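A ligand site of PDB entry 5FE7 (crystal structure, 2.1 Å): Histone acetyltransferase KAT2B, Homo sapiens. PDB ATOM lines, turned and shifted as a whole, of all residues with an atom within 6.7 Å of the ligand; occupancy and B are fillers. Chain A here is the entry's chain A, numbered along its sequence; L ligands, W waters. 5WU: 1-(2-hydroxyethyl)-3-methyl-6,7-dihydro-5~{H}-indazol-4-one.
ND2 of Asn 91 lies within hydrogen-bond range of O1 of the ligand (2.9 Å).
The backbone NH of Lys 41 sits at hydrogen-bond distance from an oxygen (O) of the ligand, 3.0 Å away.
O of Tyr 97 is in hydrogen-bond range of SG of Cys 87.
The backbone carbonyl oxygen (O) of Pro 46 is in hydrogen-bond range of the side-chain hydroxyl (OH) of Tyr 90.
ND2 of Asn 91 is in hydrogen-bond range of O of Cys 87, at 2.9 Å.
Merely in contact with the ligand: Glu 44 (2.9 Å), Pro 35 (3.2 Å), Val 40 (3.4 Å), Tyr 90 (3.4 Å), Ala 45 (3.4 Å), Tyr 97 (3.4 Å) and Tyr 48 (3.8 Å).
Hydrophobic or aromatic side chains that line the ligand: Pro 35, Val 40, Ala 45, Tyr 48, Tyr 90 and Tyr 97.
Along chain A the residues within 4 Å of the ligand span positions 35 to 97.
Water W1 lies within hydrogen-bond range of O of the ligand (2.6 Å) and O of Pro 39 (2.8 Å).
Water W2 lies within hydrogen-bond range of the side-chain hydroxyl (OH) of Tyr 48 (2.5 Å), an oxygen (O1) of the ligand (2.9 Å) and the backbone NH (N) of Cys 87 (3.1 Å).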
ATOM      1  N   TRP A  34      22.614   9.283  31.780  1.00  0.00           N
ATOM      2  CA  TRP A  34      22.979  10.681  31.473  1.00  0.00           C
ATOM      3  C   TRP A  34      21.955  11.484  30.658  1.00  0.00           C
ATOM      4  O   TRP A  34      21.803  12.660  30.895  1.00  0.00           O
ATOM      5  CB  TRP A  34      24.383  10.765  30.828  1.00  0.00           C
ATOM      6  CG  TRP A  34      24.512  10.034  29.585  1.00  0.00           C
ATOM      7  CD1 TRP A  34      24.911   8.715  29.448  1.00  0.00           C
ATOM      8  CD2 TRP A  34      24.183  10.490  28.282  1.00  0.00           C
ATOM      9  NE1 TRP A  34      24.861   8.344  28.139  1.00  0.00           N
ATOM     10  CE2 TRP A  34      24.449   9.422  27.392  1.00  0.00           C
ATOM     11  CE3 TRP A  34      23.666  11.684  27.778  1.00  0.00           C
ATOM     12  CZ2 TRP A  34      24.208   9.528  26.019  1.00  0.00           C
ATOM     13  CZ3 TRP A  34      23.443  11.782  26.417  1.00  0.00           C
ATOM     14  CH2 TRP A  34      23.746  10.726  25.542  1.00  0.00           C
ATOM     15  N   PRO A  35      21.200  10.844  29.763  1.00  0.00           N
ATOM     16  CA  PRO A  35      20.207  11.653  29.042  1.00  0.00           C
ATOM     17  C   PRO A  35      19.056  12.134  29.906  1.00  0.00           C
ATOM     18  O   PRO A  35      18.366  13.085  29.540  1.00  0.00           O
ATOM     19  CB  PRO A  35      19.646  10.656  28.016  1.00  0.00           C
ATOM     20  CG  PRO A  35      20.705   9.613  27.897  1.00  0.00           C
ATOM     21  CD  PRO A  35      21.223   9.461  29.280  1.00  0.00           C
ATOM     22  N   PHE A  36      18.827  11.470  31.019  1.00  0.00           N
ATOM     23  CA  PHE A  36      17.621  11.635  31.824  1.00  0.00           C
ATOM     24  C   PHE A  36      17.863  12.436  33.105  1.00  0.00           C
ATOM     25  O   PHE A  36      16.990  12.539  33.947  1.00  0.00           O
ATOM     26  CB  PHE A  36      17.059  10.268  32.165  1.00  0.00           C
ATOM     27  CG  PHE A  36      16.941   9.356  30.947  1.00  0.00           C
ATOM     28  CD1 PHE A  36      16.147   9.699  29.906  1.00  0.00           C
ATOM     29  CD2 PHE A  36      17.743   8.249  30.820  1.00  0.00           C
ATOM     30  CE1 PHE A  36      16.123   8.954  28.727  1.00  0.00           C
ATOM     31  CE2 PHE A  36      17.730   7.484  29.662  1.00  0.00           C
ATOM     32  CZ  PHE A  36      16.914   7.827  28.617  1.00  0.00           C
ATOM     33  N   GLU A  38      18.329  15.649  33.581  1.00  0.00           N
ATOM     34  CA  GLU A  38      17.599  16.889  33.696  1.00  0.00           C
ATOM     35  C   GLU A  38      16.436  16.958  32.743  1.00  0.00           C
ATOM     36  O   GLU A  38      16.423  16.243  31.791  1.00  0.00           O
ATOM     37  CB  GLU A  38      18.588  18.040  33.399  1.00  0.00           C
ATOM     38  CG  GLU A  38      19.337  18.395  34.669  1.00  0.00           C
ATOM     39  CD  GLU A  38      20.423  19.415  34.477  1.00  0.00           C
ATOM     40  OE1 GLU A  38      20.322  20.261  33.571  1.00  0.00           O
ATOM     41  OE2 GLU A  38      21.401  19.359  35.253  1.00  0.00           O
ATOM     42  N   PRO A  39      15.514  17.902  32.959  1.00  0.00           N
ATOM     43  CA  PRO A  39      14.412  18.095  32.046  1.00  0.00           C
ATOM     44  C   PRO A  39      14.852  18.274  30.597  1.00  0.00           C
ATOM     45  O   PRO A  39      15.852  18.944  30.323  1.00  0.00           O
ATOM     46  CB  PRO A  39      13.790  19.419  32.539  1.00  0.00           C
ATOM     47  CG  PRO A  39      14.124  19.501  34.000  1.00  0.00           C
ATOM     48  CD  PRO A  39      15.444  18.813  34.131  1.00  0.00           C
ATOM     49  N   VAL A  40      14.076  17.702  29.674  1.00  0.00           N
ATOM     50  CA  VAL A  40      14.281  17.959  28.256  1.00  0.00           C
ATOM     51  C   VAL A  40      14.196  19.458  28.025  1.00  0.00           C
ATOM     52  O   VAL A  40      13.363  20.104  28.622  1.00  0.00           O
ATOM     53  CB  VAL A  40      13.213  17.236  27.437  1.00  0.00           C
ATOM     54  CG1 VAL A  40      13.317  17.597  25.960  1.00  0.00           C
ATOM     55  CG2 VAL A  40      13.344  15.729  27.638  1.00  0.00           C
ATOM     56  N   LYS A  41      15.088  20.029  27.215  1.00  0.00           N
ATOM     57  CA  LYS A  41      15.052  21.491  27.006  1.00  0.00           C
ATOM     58  C   LYS A  41      14.232  21.805  25.777  1.00  0.00           C
ATOM     59  O   LYS A  41      14.502  21.249  24.679  1.00  0.00           O
ATOM     60  CB  LYS A  41      16.427  22.094  26.798  1.00  0.00           C
ATOM     61  CG  LYS A  41      17.316  22.012  27.988  1.00  0.00           C
ATOM     62  CD  LYS A  41      18.519  22.937  27.780  1.00  0.00           C
ATOM     63  CE  LYS A  41      19.822  22.366  28.324  1.00  0.00           C
ATOM     64  NZ  LYS A  41      19.637  21.312  29.386  1.00  0.00           N
ATOM     65  N   ARG A  42      13.237  22.665  25.967  1.00  0.00           N
ATOM     66  CA  ARG A  42      12.315  23.011  24.898  1.00  0.00           C
ATOM     67  C   ARG A  42      13.070  23.526  23.677  1.00  0.00           C
ATOM     68  O   ARG A  42      12.771  23.139  22.536  1.00  0.00           O
ATOM     69  CB  ARG A  42      11.291  24.043  25.408  1.00  0.00           C
ATOM     70  CG  ARG A  42      10.445  24.662  24.304  1.00  0.00           C
ATOM     71  CD  ARG A  42       9.359  25.620  24.771  1.00  0.00           C
ATOM     72  NE  ARG A  42       8.083  24.965  25.036  1.00  0.00           N
ATOM     73  CZ  ARG A  42       7.648  24.494  26.211  1.00  0.00           C
ATOM     74  NH1 ARG A  42       8.375  24.531  27.323  1.00  0.00           N
ATOM     75  NH2 ARG A  42       6.441  23.942  26.242  1.00  0.00           N
ATOM     76  N   GLU A  44      15.836  22.717  22.597  1.00  0.00           N
ATOM     77  CA  GLU A  44      16.510  21.647  21.858  1.00  0.00           C
ATOM     78  C   GLU A  44      15.588  20.603  21.324  1.00  0.00           C
ATOM     79  O   GLU A  44      16.034  19.760  20.570  1.00  0.00           O
ATOM     80  CB  GLU A  44      17.516  20.977  22.756  1.00  0.00           C
ATOM     81  CG  GLU A  44      18.691  21.883  23.064  1.00  0.00           C
ATOM     82  CD  GLU A  44      19.388  21.515  24.355  1.00  0.00           C
ATOM     83  OE1 GLU A  44      19.704  22.448  25.125  1.00  0.00           O
ATOM     84  OE2 GLU A  44      19.616  20.305  24.609  1.00  0.00           O
ATOM     85  N   ALA A  45      14.327  20.585  21.703  1.00  0.00           N
ATOM     86  CA  ALA A  45      13.492  19.488  21.207  1.00  0.00           C
ATOM     87  C   ALA A  45      12.169  19.906  20.638  1.00  0.00           C
ATOM     88  O   ALA A  45      11.181  19.969  21.388  1.00  0.00           O
ATOM     89  CB  ALA A  45      13.300  18.453  22.276  1.00  0.00           C
ATOM     90  N   PRO A  46      12.125  20.135  19.303  1.00  0.00           N
ATOM     91  CA  PRO A  46      10.973  20.883  18.765  1.00  0.00           C
ATOM     92  C   PRO A  46       9.670  20.143  18.938  1.00  0.00           C
ATOM     93  O   PRO A  46       9.579  18.941  18.631  1.00  0.00           O
ATOM     94  CB  PRO A  46      11.313  21.093  17.246  1.00  0.00           C
ATOM     95  CG  PRO A  46      12.662  20.482  17.044  1.00  0.00           C
ATOM     96  CD  PRO A  46      12.980  19.589  18.222  1.00  0.00           C
ATOM     97  N   TYR A  48       8.507  18.896  21.539  1.00  0.00           N
ATOM     98  CA  TYR A  48       8.511  17.871  22.586  1.00  0.00           C
ATOM     99  C   TYR A  48       7.383  18.088  23.590  1.00  0.00           C
ATOM    100  O   TYR A  48       6.653  17.163  23.908  1.00  0.00           O
ATOM    101  CB  TYR A  48       9.824  17.862  23.350  1.00  0.00           C
ATOM    102  CG  TYR A  48       9.906  16.790  24.379  1.00  0.00           C
ATOM    103  CD1 TYR A  48      10.372  15.535  24.032  1.00  0.00           C
ATOM    104  CD2 TYR A  48       9.541  17.011  25.706  1.00  0.00           C
ATOM    105  CE1 TYR A  48      10.494  14.531  24.978  1.00  0.00           C
ATOM    106  CE2 TYR A  48       9.657  16.017  26.660  1.00  0.00           C
ATOM    107  CZ  TYR A  48      10.117  14.771  26.285  1.00  0.00           C
ATOM    108  OH  TYR A  48      10.277  13.749  27.232  1.00  0.00           O
ATOM    109  N   VAL A  83       9.745   8.276  32.537  1.00  0.00           N
ATOM    110  CA  VAL A  83      10.973   8.775  31.972  1.00  0.00           C
ATOM    111  C   VAL A  83      11.324   7.954  30.702  1.00  0.00           C
ATOM    112  O   VAL A  83      11.742   8.500  29.648  1.00  0.00           O
ATOM    113  CB  VAL A  83      12.110   8.629  33.006  1.00  0.00           C
ATOM    114  CG1 VAL A  83      13.462   8.920  32.359  1.00  0.00           C
ATOM    115  CG2 VAL A  83      11.909   9.553  34.172  1.00  0.00           C
ATOM    116  N   ASN A  86       8.340   8.191  27.765  1.00  0.00           N
ATOM    117  CA  ASN A  86       8.417   9.507  27.076  1.00  0.00           C
ATOM    118  C   ASN A  86       9.532   9.498  26.048  1.00  0.00           C
ATOM    119  O   ASN A  86       9.353   9.817  24.862  1.00  0.00           O
ATOM    120  CB  ASN A  86       8.689  10.618  28.082  1.00  0.00           C
ATOM    121  CG  ASN A  86       7.512  10.948  28.967  1.00  0.00           C
ATOM    122  OD1 ASN A  86       6.383  10.520  28.747  1.00  0.00           O
ATOM    123  ND2 ASN A  86       7.783  11.759  29.975  1.00  0.00           N
ATOM    124  N   CYS A  87      10.689   9.056  26.490  1.00  0.00           N
ATOM    125  CA  CYS A  87      11.853   9.026  25.606  1.00  0.00           C
ATOM    126  C   CYS A  87      11.575   8.115  24.374  1.00  0.00           C
ATOM    127  O   CYS A  87      11.903   8.481  23.224  1.00  0.00           O
ATOM    128  CB  CYS A  87      13.038   8.530  26.384  1.00  0.00           C
ATOM    129  SG  CYS A  87      14.519   8.412  25.405  1.00  0.00           S
ATOM    130  N   LYS A  88      10.941   6.971  24.615  1.00  0.00           N
ATOM    131  CA  LYS A  88      10.764   5.991  23.527  1.00  0.00           C
ATOM    132  C   LYS A  88       9.721   6.417  22.605  1.00  0.00           C
ATOM    133  O   LYS A  88       9.794   6.098  21.429  1.00  0.00           O
ATOM    134  CB  LYS A  88      10.449   4.596  24.076  1.00  0.00           C
ATOM    135  CG  LYS A  88      11.696   3.984  24.655  1.00  0.00           C
ATOM    136  CD  LYS A  88      11.470   2.504  24.998  1.00  0.00           C
ATOM    137  CE  LYS A  88      11.239   2.297  26.446  1.00  0.00           C
ATOM    138  NZ  LYS A  88      10.629   0.965  26.729  1.00  0.00           N
ATOM    139  N   TYR A  90       9.171   9.580  21.792  1.00  0.00           N
ATOM    140  CA  TYR A  90       9.610  10.782  21.051  1.00  0.00           C
ATOM    141  C   TYR A  90      10.774  10.509  20.108  1.00  0.00           C
ATOM    142  O   TYR A  90      10.816  11.005  19.038  1.00  0.00           O
ATOM    143  CB  TYR A  90       9.967  11.918  22.055  1.00  0.00           C
ATOM    144  CG  TYR A  90      10.221  13.233  21.356  1.00  0.00           C
ATOM    145  CD1 TYR A  90       9.162  14.040  20.906  1.00  0.00           C
ATOM    146  CD2 TYR A  90      11.523  13.649  21.099  1.00  0.00           C
ATOM    147  CE1 TYR A  90       9.425  15.236  20.225  1.00  0.00           C
ATOM    148  CE2 TYR A  90      11.789  14.846  20.433  1.00  0.00           C
ATOM    149  CZ  TYR A  90      10.756  15.625  20.001  1.00  0.00           C
ATOM    150  OH  TYR A  90      11.080  16.807  19.375  1.00  0.00           O
ATOM    151  N   ASN A  91      11.733   9.715  20.526  1.00  0.00           N
ATOM    152  CA  ASN A  91      12.954   9.553  19.768  1.00  0.00           C
ATOM    153  C   ASN A  91      12.922   8.365  18.795  1.00  0.00           C
ATOM    154  O   ASN A  91      12.215   7.398  19.031  1.00  0.00           O
ATOM    155  CB  ASN A  91      14.091   9.416  20.765  1.00  0.00           C
ATOM    156  CG  ASN A  91      14.269  10.685  21.607  1.00  0.00           C
ATOM    157  OD1 ASN A  91      14.812  11.655  21.148  1.00  0.00           O
ATOM    158  ND2 ASN A  91      13.753  10.692  22.808  1.00  0.00           N
ATOM    159  N   TYR A  97      19.384   7.961  22.504  1.00  0.00           N
ATOM    160  CA  TYR A  97      18.504   8.157  23.644  1.00  0.00           C
ATOM    161  C   TYR A  97      17.631   6.929  23.853  1.00  0.00           C
ATOM    162  O   TYR A  97      17.473   6.500  24.977  1.00  0.00           O
ATOM    163  CB  TYR A  97      17.645   9.431  23.536  1.00  0.00           C
ATOM    164  CG  TYR A  97      18.411  10.783  23.519  1.00  0.00           C
ATOM    165  CD1 TYR A  97      19.598  10.974  24.195  1.00  0.00           C
ATOM    166  CD2 TYR A  97      17.899  11.856  22.776  1.00  0.00           C
ATOM    167  CE1 TYR A  97      20.285  12.209  24.113  1.00  0.00           C
ATOM    168  CE2 TYR A  97      18.560  13.068  22.664  1.00  0.00           C
ATOM    169  CZ  TYR A  97      19.752  13.259  23.332  1.00  0.00           C
ATOM    170  OH  TYR A  97      20.353  14.517  23.213  1.00  0.00           O
HETATM  171  C4  5WU L   1      16.763  14.721  25.395  1.00  0.00           C
HETATM  172  C5  5WU L   1      15.584  14.276  24.861  1.00  0.00           C
HETATM  173  C6  5WU L   1      14.872  13.120  25.375  1.00  0.00           C
HETATM  174  N1  5WU L   1      17.137  15.788  24.622  1.00  0.00           N
HETATM  175  C7  5WU L   1      15.447  12.442  26.596  1.00  0.00           C
HETATM  176  C8  5WU L   1      16.970  12.638  26.750  1.00  0.00           C
HETATM  177  C9  5WU L   1      17.419  14.107  26.598  1.00  0.00           C
HETATM  178  O1  5WU L   1      13.817  12.732  24.866  1.00  0.00           O
HETATM  179  C1  5WU L   1      15.313  15.146  23.776  1.00  0.00           C
HETATM  180  C   5WU L   1      14.120  15.205  22.887  1.00  0.00           C
HETATM  181  N   5WU L   1      16.261  16.040  23.622  1.00  0.00           N
HETATM  182  C2  5WU L   1      18.252  16.716  24.803  1.00  0.00           C
HETATM  183  C3  5WU L   1      17.803  18.097  25.270  1.00  0.00           C
HETATM  184  O   5WU L   1      17.232  18.056  26.591  1.00  0.00           O
HETATM  185  O   HOH W   1      18.050  17.734  28.986  1.00  0.00           O
HETATM  186  O   HOH W   2      11.866  11.907  26.794  1.00  0.00           O
